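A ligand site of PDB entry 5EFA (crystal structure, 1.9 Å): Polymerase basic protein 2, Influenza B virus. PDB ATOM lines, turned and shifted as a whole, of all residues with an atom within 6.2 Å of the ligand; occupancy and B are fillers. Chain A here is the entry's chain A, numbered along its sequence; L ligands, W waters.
The side-chain hydroxyl of Tyr 116 is in hydrogen-bond range of an oxygen (O9) of the ligand. The side-chain carboxylate (OE2) of Glu 45 sits at hydrogen-bond distance from a nitrogen (N4) of the ligand (2.7 Å). NZ of Lys 60 lies within hydrogen-bond range of O14 of the ligand. An oxygen (O12) of the ligand lies within hydrogen-bond range of the side-chain amide nitrogen (NE2) of Gln 7 (3.0 Å). The indole nitrogen of Trp 41 lies close to a nitrogen (N2) of the ligand (3.4 Å). An oxygen (O3) of the ligand is in salt-bridge range of the side-chain amino group (NZ) of Lys 23 (3.1 Å).
The backbone carbonyl oxygen of Glu 45 lies within hydrogen-bond range of the backbone NH of Lys 60 (2.9 Å). The side-chain carboxylate (OE2) of Glu 45 is in salt-bridge range of the guanidinium group (NH2) of Arg 16, at 2.8 Å. The side-chain carboxylate (OE2) of Glu 45 is in hydrogen-bond range of the backbone NH (N) of Gly 21 (2.9 Å). The backbone NH (N) of Gln 7 sits at hydrogen-bond distance from the backbone carbonyl oxygen (O) of Leu 14 (2.9 Å). N of Trp 41 lies within hydrogen-bond range of OE1 of Gln 90 (3.1 Å). NE2 of Gln 90 is in hydrogen-bond range of SD of Met 115. NE2 of Gln 90 is in hydrogen-bond range of O of Gly 39, 2.9 Å away.
Arg 8 touches the ligand. Arg 16 touches the ligand (NH2 to N4, 3.8 Å). Phe 47 touches the ligand. Phe 88 touches the ligand (O to C7, 3.2 Å). Gln 90 touches the ligand (CD to C7, 3.8 Å). 11 residues have an atom within 4 Å of the ligand: Gln 7, Arg 8, Arg 16, Lys 23, Trp 41, Glu 45, Phe 47, Lys 60, Phe 88, Gln 90 and Tyr 116.
Water W2 lies within hydrogen-bond range of O2 of the ligand and NE1 of Trp 41. Water W1 lies within hydrogen-bond range of O8 of the ligand and OG of Ser 113. Water W3 lies within hydrogen-bond range of O13 of the ligand (2.8 Å) and NE2 of Gln 7 (2.8 Å).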
ATOM      1  N   GLN A   7     -14.542 -14.223  26.008  1.00  0.00           N
ATOM      2  CA  GLN A   7     -14.963 -12.975  25.387  1.00  0.00           C
ATOM      3  C   GLN A   7     -14.827 -11.834  26.403  1.00  0.00           C
ATOM      4  O   GLN A   7     -14.729 -12.061  27.610  1.00  0.00           O
ATOM      5  CB  GLN A   7     -16.376 -13.078  24.883  1.00  0.00           C
ATOM      6  CG  GLN A   7     -16.587 -14.245  23.923  1.00  0.00           C
ATOM      7  CD  GLN A   7     -18.036 -14.391  23.514  1.00  0.00           C
ATOM      8  OE1 GLN A   7     -18.838 -14.972  24.251  1.00  0.00           O
ATOM      9  NE2 GLN A   7     -18.377 -13.874  22.346  1.00  0.00           N
ATOM     10  N   ARG A   8     -14.801 -10.595  25.913  1.00  0.00           N
ATOM     11  CA  ARG A   8     -14.567  -9.478  26.808  1.00  0.00           C
ATOM     12  C   ARG A   8     -15.572  -8.389  26.534  1.00  0.00           C
ATOM     13  O   ARG A   8     -15.933  -8.140  25.389  1.00  0.00           O
ATOM     14  CB  ARG A   8     -13.137  -8.937  26.638  1.00  0.00           C
ATOM     15  CG  ARG A   8     -12.066  -9.793  27.314  1.00  0.00           C
ATOM     16  CD  ARG A   8     -10.669  -9.307  26.978  1.00  0.00           C
ATOM     17  NE  ARG A   8      -9.721 -10.419  26.833  1.00  0.00           N
ATOM     18  CZ  ARG A   8      -8.414 -10.331  27.051  1.00  0.00           C
ATOM     19  NH1 ARG A   8      -7.880  -9.183  27.420  1.00  0.00           N
ATOM     20  NH2 ARG A   8      -7.639 -11.402  26.880  1.00  0.00           N
ATOM     21  N   PHE A   9     -16.058  -7.779  27.604  1.00  0.00           N
ATOM     22  CA  PHE A   9     -16.913  -6.623  27.479  1.00  0.00           C
ATOM     23  C   PHE A   9     -16.326  -5.577  28.423  1.00  0.00           C
ATOM     24  O   PHE A   9     -16.690  -5.499  29.574  1.00  0.00           O
ATOM     25  CB  PHE A   9     -18.377  -6.965  27.813  1.00  0.00           C
ATOM     26  CG  PHE A   9     -19.300  -5.773  27.805  1.00  0.00           C
ATOM     27  CD1 PHE A   9     -19.385  -4.932  26.688  1.00  0.00           C
ATOM     28  CD2 PHE A   9     -20.081  -5.476  28.921  1.00  0.00           C
ATOM     29  CE1 PHE A   9     -20.240  -3.818  26.693  1.00  0.00           C
ATOM     30  CE2 PHE A   9     -20.939  -4.379  28.926  1.00  0.00           C
ATOM     31  CZ  PHE A   9     -21.010  -3.541  27.807  1.00  0.00           C
ATOM     32  N   GLY A  10     -15.333  -4.832  27.919  1.00  0.00           N
ATOM     33  CA  GLY A  10     -14.572  -3.950  28.783  1.00  0.00           C
ATOM     34  C   GLY A  10     -13.902  -4.749  29.890  1.00  0.00           C
ATOM     35  O   GLY A  10     -13.142  -5.692  29.615  1.00  0.00           O
ATOM     36  N   LEU A  14     -16.009 -13.063  30.065  1.00  0.00           N
ATOM     37  CA  LEU A  14     -17.106 -14.016  30.100  1.00  0.00           C
ATOM     38  C   LEU A  14     -16.844 -15.250  29.240  1.00  0.00           C
ATOM     39  O   LEU A  14     -16.134 -15.176  28.220  1.00  0.00           O
ATOM     40  CB  LEU A  14     -18.392 -13.316  29.664  1.00  0.00           C
ATOM     41  CG  LEU A  14     -18.193 -12.517  28.381  1.00  0.00           C
ATOM     42  CD1 LEU A  14     -18.772 -13.259  27.190  1.00  0.00           C
ATOM     43  CD2 LEU A  14     -18.658 -11.076  28.448  1.00  0.00           C
ATOM     44  N   ARG A  16     -19.417 -18.456  27.724  1.00  0.00           N
ATOM     45  CA  ARG A  16     -20.766 -18.998  27.689  1.00  0.00           C
ATOM     46  C   ARG A  16     -20.765 -20.477  28.059  1.00  0.00           C
ATOM     47  O   ARG A  16     -19.952 -21.255  27.531  1.00  0.00           O
ATOM     48  CB  ARG A  16     -21.424 -18.798  26.326  1.00  0.00           C
ATOM     49  CG  ARG A  16     -22.893 -19.246  26.304  1.00  0.00           C
ATOM     50  CD  ARG A  16     -23.570 -18.889  24.985  1.00  0.00           C
ATOM     51  NE  ARG A  16     -23.011 -19.649  23.875  1.00  0.00           N
ATOM     52  CZ  ARG A  16     -23.368 -19.492  22.608  1.00  0.00           C
ATOM     53  NH1 ARG A  16     -22.796 -20.228  21.666  1.00  0.00           N
ATOM     54  NH2 ARG A  16     -24.288 -18.596  22.286  1.00  0.00           N
ATOM     55  N   GLY A  21     -27.622 -17.797  21.745  1.00  0.00           N
ATOM     56  CA  GLY A  21     -28.168 -16.498  21.392  1.00  0.00           C
ATOM     57  C   GLY A  21     -27.992 -16.133  19.929  1.00  0.00           C
ATOM     58  O   GLY A  21     -27.086 -16.646  19.262  1.00  0.00           O
ATOM     59  N   LYS A  23     -27.979 -12.476  17.485  1.00  0.00           N
ATOM     60  CA  LYS A  23     -27.906 -11.019  17.549  1.00  0.00           C
ATOM     61  C   LYS A  23     -28.717 -10.391  16.416  1.00  0.00           C
ATOM     62  O   LYS A  23     -28.567 -10.780  15.273  1.00  0.00           O
ATOM     63  CB  LYS A  23     -26.451 -10.555  17.484  1.00  0.00           C
ATOM     64  CG  LYS A  23     -26.256  -9.075  17.802  1.00  0.00           C
ATOM     65  CD  LYS A  23     -24.790  -8.689  17.715  1.00  0.00           C
ATOM     66  CE  LYS A  23     -24.316  -8.655  16.280  1.00  0.00           C
ATOM     67  NZ  LYS A  23     -23.068  -7.861  16.159  1.00  0.00           N
ATOM     68  N   GLY A  39     -27.016  -4.127  18.815  1.00  0.00           N
ATOM     69  CA  GLY A  39     -27.185  -5.519  18.464  1.00  0.00           C
ATOM     70  C   GLY A  39     -27.742  -6.228  19.687  1.00  0.00           C
ATOM     71  O   GLY A  39     -27.021  -6.517  20.641  1.00  0.00           O
ATOM     72  N   TRP A  41     -29.205  -9.306  21.697  1.00  0.00           N
ATOM     73  CA  TRP A  41     -29.152 -10.765  21.678  1.00  0.00           C
ATOM     74  C   TRP A  41     -30.453 -11.389  22.169  1.00  0.00           C
ATOM     75  O   TRP A  41     -31.038 -10.964  23.176  1.00  0.00           O
ATOM     76  CB  TRP A  41     -27.977 -11.249  22.520  1.00  0.00           C
ATOM     77  CG  TRP A  41     -26.658 -10.925  21.886  1.00  0.00           C
ATOM     78  CD1 TRP A  41     -26.008  -9.737  21.881  1.00  0.00           C
ATOM     79  CD2 TRP A  41     -25.837 -11.838  21.143  1.00  0.00           C
ATOM     80  NE1 TRP A  41     -24.822  -9.839  21.178  1.00  0.00           N
ATOM     81  CE2 TRP A  41     -24.704 -11.121  20.713  1.00  0.00           C
ATOM     82  CE3 TRP A  41     -25.969 -13.178  20.779  1.00  0.00           C
ATOM     83  CZ2 TRP A  41     -23.692 -11.718  19.953  1.00  0.00           C
ATOM     84  CZ3 TRP A  41     -24.967 -13.761  20.029  1.00  0.00           C
ATOM     85  CH2 TRP A  41     -23.844 -13.037  19.618  1.00  0.00           C
ATOM     86  N   ASP A  42     -30.894 -12.415  21.451  1.00  0.00           N
ATOM     87  CA  ASP A  42     -32.146 -13.123  21.739  1.00  0.00           C
ATOM     88  C   ASP A  42     -31.828 -14.570  22.123  1.00  0.00           C
ATOM     89  O   ASP A  42     -31.009 -15.207  21.476  1.00  0.00           O
ATOM     90  CB  ASP A  42     -33.060 -13.079  20.503  1.00  0.00           C
ATOM     91  CG  ASP A  42     -34.508 -13.401  20.827  1.00  0.00           C
ATOM     92  OD1 ASP A  42     -34.774 -13.924  21.920  1.00  0.00           O
ATOM     93  OD2 ASP A  42     -35.373 -13.120  19.972  1.00  0.00           O
ATOM     94  N   GLU A  45     -29.366 -17.690  27.749  1.00  0.00           N
ATOM     95  CA  GLU A  45     -27.951 -18.051  27.799  1.00  0.00           C
ATOM     96  C   GLU A  45     -27.454 -17.985  29.231  1.00  0.00           C
ATOM     97  O   GLU A  45     -27.989 -17.225  30.027  1.00  0.00           O
ATOM     98  CB  GLU A  45     -27.109 -17.128  26.906  1.00  0.00           C
ATOM     99  CG  GLU A  45     -27.436 -17.215  25.415  1.00  0.00           C
ATOM    100  CD  GLU A  45     -26.626 -16.239  24.576  1.00  0.00           C
ATOM    101  OE1 GLU A  45     -26.823 -15.013  24.737  1.00  0.00           O
ATOM    102  OE2 GLU A  45     -25.795 -16.711  23.766  1.00  0.00           O
ATOM    103  N   PHE A  47     -23.699 -17.617  31.454  1.00  0.00           N
ATOM    104  CA  PHE A  47     -22.280 -17.328  31.332  1.00  0.00           C
ATOM    105  C   PHE A  47     -21.526 -17.476  32.644  1.00  0.00           C
ATOM    106  O   PHE A  47     -22.034 -17.162  33.715  1.00  0.00           O
ATOM    107  CB  PHE A  47     -22.047 -15.900  30.817  1.00  0.00           C
ATOM    108  CG  PHE A  47     -22.634 -15.626  29.483  1.00  0.00           C
ATOM    109  CD1 PHE A  47     -23.967 -15.275  29.373  1.00  0.00           C
ATOM    110  CD2 PHE A  47     -21.863 -15.692  28.342  1.00  0.00           C
ATOM    111  CE1 PHE A  47     -24.524 -15.015  28.141  1.00  0.00           C
ATOM    112  CE2 PHE A  47     -22.425 -15.418  27.107  1.00  0.00           C
ATOM    113  CZ  PHE A  47     -23.758 -15.085  27.022  1.00  0.00           C
ATOM    114  N   LYS A  60     -29.138 -14.981  31.481  1.00  0.00           N
ATOM    115  CA  LYS A  60     -29.892 -13.906  30.824  1.00  0.00           C
ATOM    116  C   LYS A  60     -30.836 -14.448  29.747  1.00  0.00           C
ATOM    117  O   LYS A  60     -30.674 -15.568  29.266  1.00  0.00           O
ATOM    118  CB  LYS A  60     -28.926 -12.888  30.189  1.00  0.00           C
ATOM    119  CG  LYS A  60     -28.221 -13.433  28.924  1.00  0.00           C
ATOM    120  CD  LYS A  60     -27.383 -12.377  28.234  1.00  0.00           C
ATOM    121  CE  LYS A  60     -28.251 -11.241  27.691  1.00  0.00           C
ATOM    122  NZ  LYS A  60     -28.816 -11.512  26.343  1.00  0.00           N
ATOM    123  N   VAL A  87     -25.440  -4.373  32.556  1.00  0.00           N
ATOM    124  CA  VAL A  87     -25.274  -3.743  31.233  1.00  0.00           C
ATOM    125  C   VAL A  87     -25.181  -4.798  30.137  1.00  0.00           C
ATOM    126  O   VAL A  87     -25.853  -4.694  29.091  1.00  0.00           O
ATOM    127  CB  VAL A  87     -24.022  -2.844  31.190  1.00  0.00           C
ATOM    128  CG1 VAL A  87     -23.835  -2.306  29.759  1.00  0.00           C
ATOM    129  CG2 VAL A  87     -24.153  -1.657  32.213  1.00  0.00           C
ATOM    130  N   PHE A  88     -24.359  -5.814  30.370  1.00  0.00           N
ATOM    131  CA  PHE A  88     -24.168  -6.891  29.393  1.00  0.00           C
ATOM    132  C   PHE A  88     -25.484  -7.588  29.025  1.00  0.00           C
ATOM    133  O   PHE A  88     -25.699  -8.003  27.872  1.00  0.00           O
ATOM    134  CB  PHE A  88     -23.189  -7.938  29.926  1.00  0.00           C
ATOM    135  CG  PHE A  88     -22.919  -9.060  28.950  1.00  0.00           C
ATOM    136  CD1 PHE A  88     -21.926  -8.943  27.992  1.00  0.00           C
ATOM    137  CD2 PHE A  88     -23.661 -10.237  29.004  1.00  0.00           C
ATOM    138  CE1 PHE A  88     -21.658  -9.983  27.078  1.00  0.00           C
ATOM    139  CE2 PHE A  88     -23.410 -11.297  28.101  1.00  0.00           C
ATOM    140  CZ  PHE A  88     -22.419 -11.157  27.148  1.00  0.00           C
ATOM    141  N   SER A  89     -26.360  -7.728  30.012  1.00  0.00           N
ATOM    142  CA  SER A  89     -27.619  -8.445  29.816  1.00  0.00           C
ATOM    143  C   SER A  89     -28.589  -7.642  28.947  1.00  0.00           C
ATOM    144  O   SER A  89     -29.639  -8.144  28.544  1.00  0.00           O
ATOM    145  CB  SER A  89     -28.268  -8.737  31.172  1.00  0.00           C
ATOM    146  OG  SER A  89     -28.760  -7.535  31.762  1.00  0.00           O
ATOM    147  N   GLN A  90     -28.239  -6.377  28.693  1.00  0.00           N
ATOM    148  CA  GLN A  90     -29.066  -5.451  27.913  1.00  0.00           C
ATOM    149  C   GLN A  90     -30.458  -5.324  28.541  1.00  0.00           C
ATOM    150  O   GLN A  90     -31.443  -5.122  27.842  1.00  0.00           O
ATOM    151  CB  GLN A  90     -29.156  -5.917  26.454  1.00  0.00           C
ATOM    152  CG  GLN A  90     -27.767  -6.073  25.843  1.00  0.00           C
ATOM    153  CD  GLN A  90     -27.809  -6.584  24.411  1.00  0.00           C
ATOM    154  OE1 GLN A  90     -28.532  -7.511  24.089  1.00  0.00           O
ATOM    155  NE2 GLN A  90     -27.016  -5.957  23.533  1.00  0.00           N
ATOM    156  N   SER A 113     -19.169   3.378  21.306  1.00  0.00           N
ATOM    157  CA  SER A 113     -20.392   2.754  20.802  1.00  0.00           C
ATOM    158  C   SER A 113     -21.401   2.608  21.952  1.00  0.00           C
ATOM    159  O   SER A 113     -21.003   2.610  23.112  1.00  0.00           O
ATOM    160  CB  SER A 113     -20.070   1.398  20.175  1.00  0.00           C
ATOM    161  OG  SER A 113     -19.933   0.412  21.168  1.00  0.00           O
ATOM    162  N   MET A 115     -23.179   0.351  23.666  1.00  0.00           N
ATOM    163  CA  MET A 115     -23.026  -0.575  24.805  1.00  0.00           C
ATOM    164  C   MET A 115     -21.886  -0.099  25.701  1.00  0.00           C
ATOM    165  O   MET A 115     -21.927  -0.263  26.923  1.00  0.00           O
ATOM    166  CB  MET A 115     -22.773  -2.008  24.322  1.00  0.00           C
ATOM    167  CG  MET A 115     -23.991  -2.691  23.748  1.00  0.00           C
ATOM    168  SD  MET A 115     -25.334  -2.889  24.968  1.00  0.00           S
ATOM    169  CE  MET A 115     -24.581  -4.024  26.132  1.00  0.00           C
ATOM    170  N   TYR A 116     -20.878   0.509  25.105  1.00  0.00           N
ATOM    171  CA  TYR A 116     -19.726   0.973  25.878  1.00  0.00           C
ATOM    172  C   TYR A 116     -20.008   2.321  26.536  1.00  0.00           C
ATOM    173  O   TYR A 116     -19.471   2.626  27.609  1.00  0.00           O
ATOM    174  CB  TYR A 116     -18.473   1.002  24.996  1.00  0.00           C
ATOM    175  CG  TYR A 116     -17.994  -0.410  24.775  1.00  0.00           C
ATOM    176  CD1 TYR A 116     -18.608  -1.232  23.839  1.00  0.00           C
ATOM    177  CD2 TYR A 116     -16.971  -0.945  25.558  1.00  0.00           C
ATOM    178  CE1 TYR A 116     -18.204  -2.541  23.659  1.00  0.00           C
ATOM    179  CE2 TYR A 116     -16.552  -2.263  25.384  1.00  0.00           C
ATOM    180  CZ  TYR A 116     -17.169  -3.049  24.438  1.00  0.00           C
ATOM    181  OH  TYR A 116     -16.765  -4.352  24.251  1.00  0.00           O
HETATM  182  P1  LIG L   1     -19.843  -8.618  17.968  1.00  0.00           P
HETATM  183  O1  LIG L   1     -18.921  -9.756  18.319  1.00  0.00           O
HETATM  184  O2  LIG L   1     -21.139  -8.636  18.758  1.00  0.00           O
HETATM  185  O3  LIG L   1     -20.025  -8.387  16.489  1.00  0.00           O
HETATM  186  O4  LIG L   1     -19.030  -7.310  18.451  1.00  0.00           O
HETATM  187  P2  LIG L   1     -19.668  -6.167  19.391  1.00  0.00           P
HETATM  188  O5  LIG L   1     -21.157  -6.018  19.169  1.00  0.00           O
HETATM  189  O6  LIG L   1     -18.742  -4.985  19.334  1.00  0.00           O
HETATM  190  O7  LIG L   1     -19.479  -6.898  20.802  1.00  0.00           O
HETATM  191  P3  LIG L   1     -19.471  -6.127  22.207  1.00  0.00           P
HETATM  192  O8  LIG L   1     -20.656  -5.208  22.300  1.00  0.00           O
HETATM  193  O9  LIG L   1     -18.049  -5.644  22.422  1.00  0.00           O
HETATM  194  O10 LIG L   1     -19.739  -7.373  23.190  1.00  0.00           O
HETATM  195  C1  LIG L   1     -18.636  -8.004  23.834  1.00  0.00           C
HETATM  196  C2  LIG L   1     -18.588  -9.486  23.483  1.00  0.00           C
HETATM  197  O11 LIG L   1     -19.717 -10.170  24.025  1.00  0.00           O
HETATM  198  C3  LIG L   1     -18.669  -9.723  21.984  1.00  0.00           C
HETATM  199  O12 LIG L   1     -17.965 -10.938  21.780  1.00  0.00           O
HETATM  200  C4  LIG L   1     -20.142  -9.942  21.683  1.00  0.00           C
HETATM  201  O13 LIG L   1     -20.296 -10.848  20.595  1.00  0.00           O
HETATM  202  C5  LIG L   1     -20.557 -10.644  22.958  1.00  0.00           C
HETATM  203  N1  LIG L   1     -21.941 -10.540  23.454  1.00  0.00           N
HETATM  204  C6  LIG L   1     -22.393  -9.203  23.908  1.00  0.00           C
HETATM  205  N2  LIG L   1     -23.717  -9.663  24.337  1.00  0.00           N
HETATM  206  C7  LIG L   1     -24.586  -8.585  24.919  1.00  0.00           C
HETATM  207  C8  LIG L   1     -23.958 -10.972  24.188  1.00  0.00           C
HETATM  208  C9  LIG L   1     -25.097 -11.838  24.466  1.00  0.00           C
HETATM  209  O14 LIG L   1     -26.160 -11.422  24.978  1.00  0.00           O
HETATM  210  N3  LIG L   1     -24.946 -13.130  24.157  1.00  0.00           N
HETATM  211  C10 LIG L   1     -23.818 -13.635  23.614  1.00  0.00           C
HETATM  212  N4  LIG L   1     -23.778 -14.964  23.342  1.00  0.00           N
HETATM  213  N5  LIG L   1     -22.726 -12.884  23.325  1.00  0.00           N
HETATM  214  C11 LIG L   1     -22.756 -11.575  23.595  1.00  0.00           C
HETATM  215  O   HOH W   1     -21.000  -2.852  21.049  1.00  0.00           O
HETATM  216  O   HOH W   2     -22.604  -7.775  20.499  1.00  0.00           O
HETATM  217  O   HOH W   3     -20.791 -13.546  20.967  1.00  0.00           O
HETATM  218  O   HOH W   4     -21.728 -16.285  20.956  1.00  0.00           O
